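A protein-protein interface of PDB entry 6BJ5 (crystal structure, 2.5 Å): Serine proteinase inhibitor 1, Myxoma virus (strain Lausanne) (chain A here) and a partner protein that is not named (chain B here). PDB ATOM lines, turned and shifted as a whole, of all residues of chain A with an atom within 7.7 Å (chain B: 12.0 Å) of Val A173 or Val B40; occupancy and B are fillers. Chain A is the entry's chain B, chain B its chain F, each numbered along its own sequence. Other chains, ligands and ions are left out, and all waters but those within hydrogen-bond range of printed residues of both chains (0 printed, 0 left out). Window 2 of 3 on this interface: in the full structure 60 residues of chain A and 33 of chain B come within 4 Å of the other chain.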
ATOM      1  N   PHE A 168      12.088  -2.875 -15.387  1.00  0.00           N
ATOM      2  CA  PHE A 168      13.467  -2.393 -15.490  1.00  0.00           C
ATOM      3  C   PHE A 168      13.794  -2.276 -16.971  1.00  0.00           C
ATOM      4  O   PHE A 168      13.782  -3.286 -17.685  1.00  0.00           O
ATOM      5  CB  PHE A 168      14.435  -3.373 -14.805  1.00  0.00           C
ATOM      6  CG  PHE A 168      15.847  -2.864 -14.651  1.00  0.00           C
ATOM      7  CD1 PHE A 168      16.252  -2.258 -13.468  1.00  0.00           C
ATOM      8  CD2 PHE A 168      16.791  -3.056 -15.662  1.00  0.00           C
ATOM      9  CE1 PHE A 168      17.563  -1.811 -13.303  1.00  0.00           C
ATOM     10  CE2 PHE A 168      18.097  -2.604 -15.516  1.00  0.00           C
ATOM     11  CZ  PHE A 168      18.488  -1.981 -14.329  1.00  0.00           C
ATOM     12  N   TYR A 169      14.132  -1.071 -17.427  1.00  0.00           N
ATOM     13  CA  TYR A 169      14.248  -0.788 -18.857  1.00  0.00           C
ATOM     14  C   TYR A 169      15.719  -0.786 -19.287  1.00  0.00           C
ATOM     15  O   TYR A 169      16.479   0.135 -18.961  1.00  0.00           O
ATOM     16  CB  TYR A 169      13.560   0.534 -19.204  1.00  0.00           C
ATOM     17  CG  TYR A 169      12.120   0.604 -18.731  1.00  0.00           C
ATOM     18  CD1 TYR A 169      11.115  -0.142 -19.356  1.00  0.00           C
ATOM     19  CD2 TYR A 169      11.762   1.425 -17.667  1.00  0.00           C
ATOM     20  CE1 TYR A 169       9.797  -0.087 -18.909  1.00  0.00           C
ATOM     21  CE2 TYR A 169      10.455   1.486 -17.216  1.00  0.00           C
ATOM     22  CZ  TYR A 169       9.476   0.733 -17.839  1.00  0.00           C
ATOM     23  OH  TYR A 169       8.180   0.815 -17.382  1.00  0.00           O
ATOM     24  N   SER A 170      16.121  -1.836 -19.998  1.00  0.00           N
ATOM     25  CA  SER A 170      17.467  -1.994 -20.556  1.00  0.00           C
ATOM     26  C   SER A 170      17.406  -1.826 -22.080  1.00  0.00           C
ATOM     27  O   SER A 170      17.235  -2.795 -22.825  1.00  0.00           O
ATOM     28  CB  SER A 170      18.034  -3.354 -20.163  1.00  0.00           C
ATOM     29  OG  SER A 170      19.134  -3.707 -20.974  1.00  0.00           O
ATOM     30  N   GLY A 171      17.618  -0.601 -22.542  1.00  0.00           N
ATOM     31  CA  GLY A 171      17.491  -0.323 -23.964  1.00  0.00           C
ATOM     32  C   GLY A 171      16.042  -0.530 -24.357  1.00  0.00           C
ATOM     33  O   GLY A 171      15.149   0.201 -23.903  1.00  0.00           O
ATOM     34  N   ASN A 172      15.777  -1.527 -25.204  1.00  0.00           N
ATOM     35  CA  ASN A 172      14.400  -1.830 -25.573  1.00  0.00           C
ATOM     36  C   ASN A 172      13.859  -3.063 -24.869  1.00  0.00           C
ATOM     37  O   ASN A 172      12.638  -3.261 -24.864  1.00  0.00           O
ATOM     38  CB  ASN A 172      14.225  -1.979 -27.099  1.00  0.00           C
ATOM     39  CG  ASN A 172      15.418  -2.624 -27.794  1.00  0.00           C
ATOM     40  OD1 ASN A 172      15.704  -3.806 -27.599  1.00  0.00           O
ATOM     41  ND2 ASN A 172      16.085  -1.856 -28.657  1.00  0.00           N
ATOM     42  N   VAL A 173      14.729  -3.894 -24.279  1.00  0.00           N
ATOM     43  CA  VAL A 173      14.277  -5.024 -23.474  1.00  0.00           C
ATOM     44  C   VAL A 173      13.807  -4.517 -22.117  1.00  0.00           C
ATOM     45  O   VAL A 173      14.360  -3.563 -21.558  1.00  0.00           O
ATOM     46  CB  VAL A 173      15.406  -6.061 -23.340  1.00  0.00           C
ATOM     47  CG1 VAL A 173      14.967  -7.280 -22.510  1.00  0.00           C
ATOM     48  CG2 VAL A 173      15.885  -6.471 -24.729  1.00  0.00           C
ATOM     49  N   THR A 174      12.769  -5.159 -21.575  1.00  0.00           N
ATOM     50  CA  THR A 174      12.231  -4.811 -20.267  1.00  0.00           C
ATOM     51  C   THR A 174      12.187  -6.048 -19.386  1.00  0.00           C
ATOM     52  O   THR A 174      11.928  -7.158 -19.867  1.00  0.00           O
ATOM     53  CB  THR A 174      10.848  -4.160 -20.408  1.00  0.00           C
ATOM     54  OG1 THR A 174      10.981  -2.987 -21.226  1.00  0.00           O
ATOM     55  CG2 THR A 174      10.300  -3.712 -19.042  1.00  0.00           C
ATOM     56  N   TYR A 175      12.495  -5.870 -18.102  1.00  0.00           N
ATOM     57  CA  TYR A 175      12.585  -6.997 -17.187  1.00  0.00           C
ATOM     58  C   TYR A 175      11.671  -6.741 -16.010  1.00  0.00           C
ATOM     59  O   TYR A 175      11.269  -5.606 -15.751  1.00  0.00           O
ATOM     60  CB  TYR A 175      14.020  -7.227 -16.667  1.00  0.00           C
ATOM     61  CG  TYR A 175      15.017  -7.510 -17.757  1.00  0.00           C
ATOM     62  CD1 TYR A 175      15.393  -8.816 -18.072  1.00  0.00           C
ATOM     63  CD2 TYR A 175      15.593  -6.470 -18.474  1.00  0.00           C
ATOM     64  CE1 TYR A 175      16.315  -9.064 -19.077  1.00  0.00           C
ATOM     65  CE2 TYR A 175      16.515  -6.715 -19.482  1.00  0.00           C
ATOM     66  CZ  TYR A 175      16.870  -8.003 -19.778  1.00  0.00           C
ATOM     67  OH  TYR A 175      17.794  -8.226 -20.774  1.00  0.00           O
ATOM     68  N   LYS A 176      11.381  -7.801 -15.275  1.00  0.00           N
ATOM     69  CA  LYS A 176      10.581  -7.695 -14.068  1.00  0.00           C
ATOM     70  C   LYS A 176      11.534  -7.959 -12.925  1.00  0.00           C
ATOM     71  O   LYS A 176      12.100  -9.056 -12.820  1.00  0.00           O
ATOM     72  CB  LYS A 176       9.434  -8.700 -14.038  1.00  0.00           C
ATOM     73  CG  LYS A 176       8.704  -8.689 -12.729  1.00  0.00           C
ATOM     74  CD  LYS A 176       7.609  -9.724 -12.673  1.00  0.00           C
ATOM     75  CE  LYS A 176       8.205 -11.073 -12.361  1.00  0.00           C
ATOM     76  NZ  LYS A 176       7.152 -12.098 -12.141  1.00  0.00           N
ATOM     77  N   ALA B  12      16.110   3.479  -9.568  1.00  0.00           N
ATOM     78  CA  ALA B  12      17.100   2.682 -10.281  1.00  0.00           C
ATOM     79  C   ALA B  12      16.380   1.614 -11.100  1.00  0.00           C
ATOM     80  O   ALA B  12      16.508   0.412 -10.872  1.00  0.00           O
ATOM     81  CB  ALA B  12      18.081   2.060  -9.293  1.00  0.00           C
ATOM     82  N   ASN B  13      15.584   2.085 -12.065  1.00  0.00           N
ATOM     83  CA  ASN B  13      14.861   1.195 -12.962  1.00  0.00           C
ATOM     84  C   ASN B  13      15.446   1.209 -14.365  1.00  0.00           C
ATOM     85  O   ASN B  13      14.753   0.873 -15.332  1.00  0.00           O
ATOM     86  CB  ASN B  13      13.378   1.559 -13.020  1.00  0.00           C
ATOM     87  CG  ASN B  13      13.139   2.892 -13.668  1.00  0.00           C
ATOM     88  OD1 ASN B  13      14.058   3.689 -13.826  1.00  0.00           O
ATOM     89  ND2 ASN B  13      11.913   3.116 -14.118  1.00  0.00           N
ATOM     90  N   LYS B  14      16.707   1.579 -14.480  1.00  0.00           N
ATOM     91  CA  LYS B  14      17.490   1.536 -15.703  1.00  0.00           C
ATOM     92  C   LYS B  14      18.916   1.175 -15.294  1.00  0.00           C
ATOM     93  O   LYS B  14      19.230   1.229 -14.095  1.00  0.00           O
ATOM     94  CB  LYS B  14      17.409   2.879 -16.443  1.00  0.00           C
ATOM     95  CG  LYS B  14      17.551   4.130 -15.572  1.00  0.00           C
ATOM     96  CD  LYS B  14      17.577   5.398 -16.438  1.00  0.00           C
ATOM     97  CE  LYS B  14      17.622   6.693 -15.615  1.00  0.00           C
ATOM     98  NZ  LYS B  14      16.400   6.864 -14.772  1.00  0.00           N
ATOM     99  N   PRO B  15      19.795   0.799 -16.224  1.00  0.00           N
ATOM    100  CA  PRO B  15      21.164   0.424 -15.835  1.00  0.00           C
ATOM    101  C   PRO B  15      21.822   1.461 -14.943  1.00  0.00           C
ATOM    102  O   PRO B  15      21.738   2.670 -15.183  1.00  0.00           O
ATOM    103  CB  PRO B  15      21.892   0.293 -17.178  1.00  0.00           C
ATOM    104  CG  PRO B  15      20.850  -0.135 -18.111  1.00  0.00           C
ATOM    105  CD  PRO B  15      19.570   0.572 -17.662  1.00  0.00           C
ATOM    106  N   ILE B  34      24.768  -2.826 -13.065  1.00  0.00           N
ATOM    107  CA  ILE B  34      23.572  -3.643 -13.218  1.00  0.00           C
ATOM    108  C   ILE B  34      22.793  -3.134 -14.427  1.00  0.00           C
ATOM    109  O   ILE B  34      22.184  -2.059 -14.367  1.00  0.00           O
ATOM    110  CB  ILE B  34      22.744  -3.601 -11.937  1.00  0.00           C
ATOM    111  CG1 ILE B  34      23.516  -4.352 -10.877  1.00  0.00           C
ATOM    112  CG2 ILE B  34      21.386  -4.195 -12.122  1.00  0.00           C
ATOM    113  CD1 ILE B  34      22.918  -4.179  -9.576  1.00  0.00           C
ATOM    114  N   THR B  35      22.801  -3.906 -15.520  1.00  0.00           N
ATOM    115  CA  THR B  35      22.151  -3.516 -16.763  1.00  0.00           C
ATOM    116  C   THR B  35      20.915  -4.345 -17.094  1.00  0.00           C
ATOM    117  O   THR B  35      20.238  -4.047 -18.084  1.00  0.00           O
ATOM    118  CB  THR B  35      23.128  -3.645 -17.949  1.00  0.00           C
ATOM    119  OG1 THR B  35      23.456  -5.025 -18.136  1.00  0.00           O
ATOM    120  CG2 THR B  35      24.411  -2.864 -17.733  1.00  0.00           C
ATOM    121  N   LYS B  36      20.574  -5.347 -16.292  1.00  0.00           N
ATOM    122  CA  LYS B  36      19.539  -6.282 -16.714  1.00  0.00           C
ATOM    123  C   LYS B  36      18.975  -7.011 -15.513  1.00  0.00           C
ATOM    124  O   LYS B  36      19.595  -7.070 -14.444  1.00  0.00           O
ATOM    125  CB  LYS B  36      20.074  -7.316 -17.710  1.00  0.00           C
ATOM    126  CG  LYS B  36      21.098  -8.244 -17.085  1.00  0.00           C
ATOM    127  CD  LYS B  36      21.597  -9.353 -18.014  1.00  0.00           C
ATOM    128  CE  LYS B  36      20.450 -10.286 -18.388  1.00  0.00           C
ATOM    129  NZ  LYS B  36      20.801 -11.228 -19.486  1.00  0.00           N
ATOM    130  N   GLY B  37      17.769  -7.545 -15.709  1.00  0.00           N
ATOM    131  CA  GLY B  37      17.151  -8.481 -14.795  1.00  0.00           C
ATOM    132  C   GLY B  37      17.258  -9.906 -15.295  1.00  0.00           C
ATOM    133  O   GLY B  37      18.051 -10.224 -16.187  1.00  0.00           O
ATOM    134  N   GLU B  38      16.430 -10.780 -14.726  1.00  0.00           N
ATOM    135  CA  GLU B  38      16.366 -12.169 -15.171  1.00  0.00           C
ATOM    136  C   GLU B  38      15.134 -12.458 -16.020  1.00  0.00           C
ATOM    137  O   GLU B  38      15.250 -13.024 -17.110  1.00  0.00           O
ATOM    138  CB  GLU B  38      16.413 -13.111 -13.963  1.00  0.00           C
ATOM    139  CG  GLU B  38      17.690 -12.953 -13.162  1.00  0.00           C
ATOM    140  CD  GLU B  38      18.943 -13.086 -14.035  1.00  0.00           C
ATOM    141  OE1 GLU B  38      19.057 -14.102 -14.768  1.00  0.00           O
ATOM    142  OE2 GLU B  38      19.802 -12.165 -14.001  1.00  0.00           O
ATOM    143  N   LYS B  39      13.957 -12.049 -15.558  1.00  0.00           N
ATOM    144  CA  LYS B  39      12.693 -12.378 -16.210  1.00  0.00           C
ATOM    145  C   LYS B  39      12.339 -11.281 -17.215  1.00  0.00           C
ATOM    146  O   LYS B  39      12.012 -10.155 -16.817  1.00  0.00           O
ATOM    147  CB  LYS B  39      11.604 -12.547 -15.153  1.00  0.00           C
ATOM    148  CG  LYS B  39      11.921 -13.635 -14.124  1.00  0.00           C
ATOM    149  CD  LYS B  39      10.838 -13.756 -13.048  1.00  0.00           C
ATOM    150  CE  LYS B  39      11.102 -12.846 -11.848  1.00  0.00           C
ATOM    151  NZ  LYS B  39      12.120 -13.396 -10.919  1.00  0.00           N
ATOM    152  N   VAL B  40      12.386 -11.608 -18.519  1.00  0.00           N
ATOM    153  CA  VAL B  40      12.011 -10.627 -19.544  1.00  0.00           C
ATOM    154  C   VAL B  40      10.494 -10.424 -19.545  1.00  0.00           C
ATOM    155  O   VAL B  40       9.717 -11.352 -19.295  1.00  0.00           O
ATOM    156  CB  VAL B  40      12.518 -11.062 -20.930  1.00  0.00           C
ATOM    157  CG1 VAL B  40      12.248  -9.971 -21.985  1.00  0.00           C
ATOM    158  CG2 VAL B  40      13.995 -11.389 -20.857  1.00  0.00           C
ATOM    159  N   ILE B  41      10.072  -9.199 -19.860  1.00  0.00           N
ATOM    160  CA  ILE B  41       8.679  -8.776 -19.795  1.00  0.00           C
ATOM    161  C   ILE B  41       8.292  -8.093 -21.095  1.00  0.00           C
ATOM    162  O   ILE B  41       9.121  -7.438 -21.733  1.00  0.00           O
ATOM    163  CB  ILE B  41       8.479  -7.825 -18.580  1.00  0.00           C
ATOM    164  CG1 ILE B  41       8.383  -8.623 -17.311  1.00  0.00           C
ATOM    165  CG2 ILE B  41       7.305  -6.909 -18.716  1.00  0.00           C
ATOM    166  CD1 ILE B  41       7.407  -9.718 -17.376  1.00  0.00           C
ATOM    167  N   TYR B  42       7.035  -8.272 -21.513  1.00  0.00           N
ATOM    168  CA  TYR B  42       6.494  -7.586 -22.684  1.00  0.00           C
ATOM    169  C   TYR B  42       5.275  -6.756 -22.269  1.00  0.00           C
ATOM    170  O   TYR B  42       4.741  -6.925 -21.169  1.00  0.00           O
ATOM    171  CB  TYR B  42       6.148  -8.588 -23.802  1.00  0.00           C
ATOM    172  CG  TYR B  42       7.305  -9.516 -24.152  1.00  0.00           C
ATOM    173  CD1 TYR B  42       8.327  -9.097 -25.003  1.00  0.00           C
ATOM    174  CD2 TYR B  42       7.375 -10.815 -23.633  1.00  0.00           C
ATOM    175  CE1 TYR B  42       9.392  -9.934 -25.320  1.00  0.00           C
ATOM    176  CE2 TYR B  42       8.439 -11.659 -23.946  1.00  0.00           C
ATOM    177  CZ  TYR B  42       9.436 -11.207 -24.786  1.00  0.00           C
ATOM    178  OH  TYR B  42      10.477 -12.028 -25.113  1.00  0.00           O
ATOM    179  N   ASP B  43       4.844  -5.837 -23.139  1.00  0.00           N
ATOM    180  CA  ASP B  43       3.631  -5.061 -22.876  1.00  0.00           C
ATOM    181  C   ASP B  43       3.015  -4.638 -24.205  1.00  0.00           C
ATOM    182  O   ASP B  43       3.696  -4.563 -25.232  1.00  0.00           O
ATOM    183  CB  ASP B  43       3.924  -3.838 -21.971  1.00  0.00           C
ATOM    184  CG  ASP B  43       2.694  -2.911 -21.740  1.00  0.00           C
ATOM    185  OD1 ASP B  43       2.747  -2.112 -20.783  1.00  0.00           O
ATOM    186  OD2 ASP B  43       1.689  -2.949 -22.488  1.00  0.00           O
ATOM    187  N   THR B  44       1.703  -4.384 -24.161  1.00  0.00           N
ATOM    188  CA  THR B  44       0.900  -3.851 -25.272  1.00  0.00           C
ATOM    189  C   THR B  44       1.555  -2.691 -26.015  1.00  0.00           C
ATOM    190  O   THR B  44       1.175  -2.368 -27.143  1.00  0.00           O
ATOM    191  CB  THR B  44      -0.442  -3.362 -24.742  1.00  0.00           C
ATOM    192  OG1 THR B  44      -0.921  -4.270 -23.806  1.00  0.00           O
ATOM    193  CG2 THR B  44      -1.444  -3.163 -25.840  1.00  0.00           C
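Ser A170 touches just one residue of chain B: Thr B35 (3.1 Å).
No residue of chain B comes within 4 Å of Gly A171.
No residue of chain B comes within 4 Å of Asn A172.
Thr A174 touches just these residues of chain B: Val B40 and Ile B41.
Lys A176 touches just these residues of chain B: Lys B39 (2.9 Å) and Ile B41 (3.4 Å).
Printed residues of chain A within 4 Å of Ala B12: Phe A168 (3.5 Å).
Of the printed residues of chain A, Lys B14 touches Phe A168 and Tyr A169.
Printed residues of chain A within 4 Å of Lys B36: Phe A168 and Tyr A175.
Glu B38 touches none of the printed residues of chain A.
Of the printed residues of chain A, Val B40 touches Val A173 (3.9 Å), Thr A174 (3.5 Å) and Tyr A175 (3.7 Å).
Thr B44 touches none of the printed residues of chain A.
The nearest residue of chain A that does not touch Val B40 is Lys A176 (5.1 Å).
The backbone NH (N) of Tyr A169 lies within hydrogen-bond range of the backbone carbonyl oxygen (O) of Asn B13 (2.9 Å).
The side-chain hydroxyl (OG) of Ser A170 lies close to the backbone carbonyl oxygen (O) of Thr B35 (3.1 Å).
O of Thr A174 sits at hydrogen-bond distance from N of Ile B41.
The backbone carbonyl oxygen (O) of Lys B39 lies within hydrogen-bond range of the backbone NH (N) of Lys A176 (2.9 Å).
Of the 9 printed residues of chain A, 7 touch a printed residue of chain B.
Printed residues of chain A that touch a printed residue of chain B: Phe A168, Tyr A169, Ser A170, Val A173, Thr A174, Tyr A175 and Lys A176.
Hydrophobic or aromatic side chains of chain A within 4 Å of the printed part of chain B: Phe A168, Tyr A169, Val A173 and Tyr A175.
Of the 15 printed residues of chain B, 11 touch a printed residue of chain A.
Hydrophobic or aromatic side chains of chain B that line the printed part of chain A: Pro B15, Val B40 and Ile B41.
Among the printed residues, no Asp or Glu carboxylate lies within 4 Å of a Lys or Arg side-chain nitrogen of the other chain.
Phe A168 touches Asn B13 (CA to O, 3.5 Å).
CZ of Phe A168 touches N of Pro B15, at 3.6 Å.
O of Ile B34 touches CZ of Phe A168, at 3.7 Å.
Phe A168 touches Thr B35 (CE2 to O, 3.6 Å).
CE2 of Phe A168 touches N of Lys B36, 3.8 Å away.
Val A173 touches Val B40 (CG1 to CG1, 3.9 Å).
CZ of Tyr A175 touches CB of Lys B36 (3.9 Å).
Gly B37 touches Tyr A175 (N to CG, 3.4 Å).
Tyr A175 touches Lys B39 (CA to O, 3.2 Å).
Tyr A175 touches Val B40.
The backbone carbonyl oxygen (O) of Tyr A175 lies within hydrogen-bond range of the backbone NH (N) of Phe A168, at 2.9 Å.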
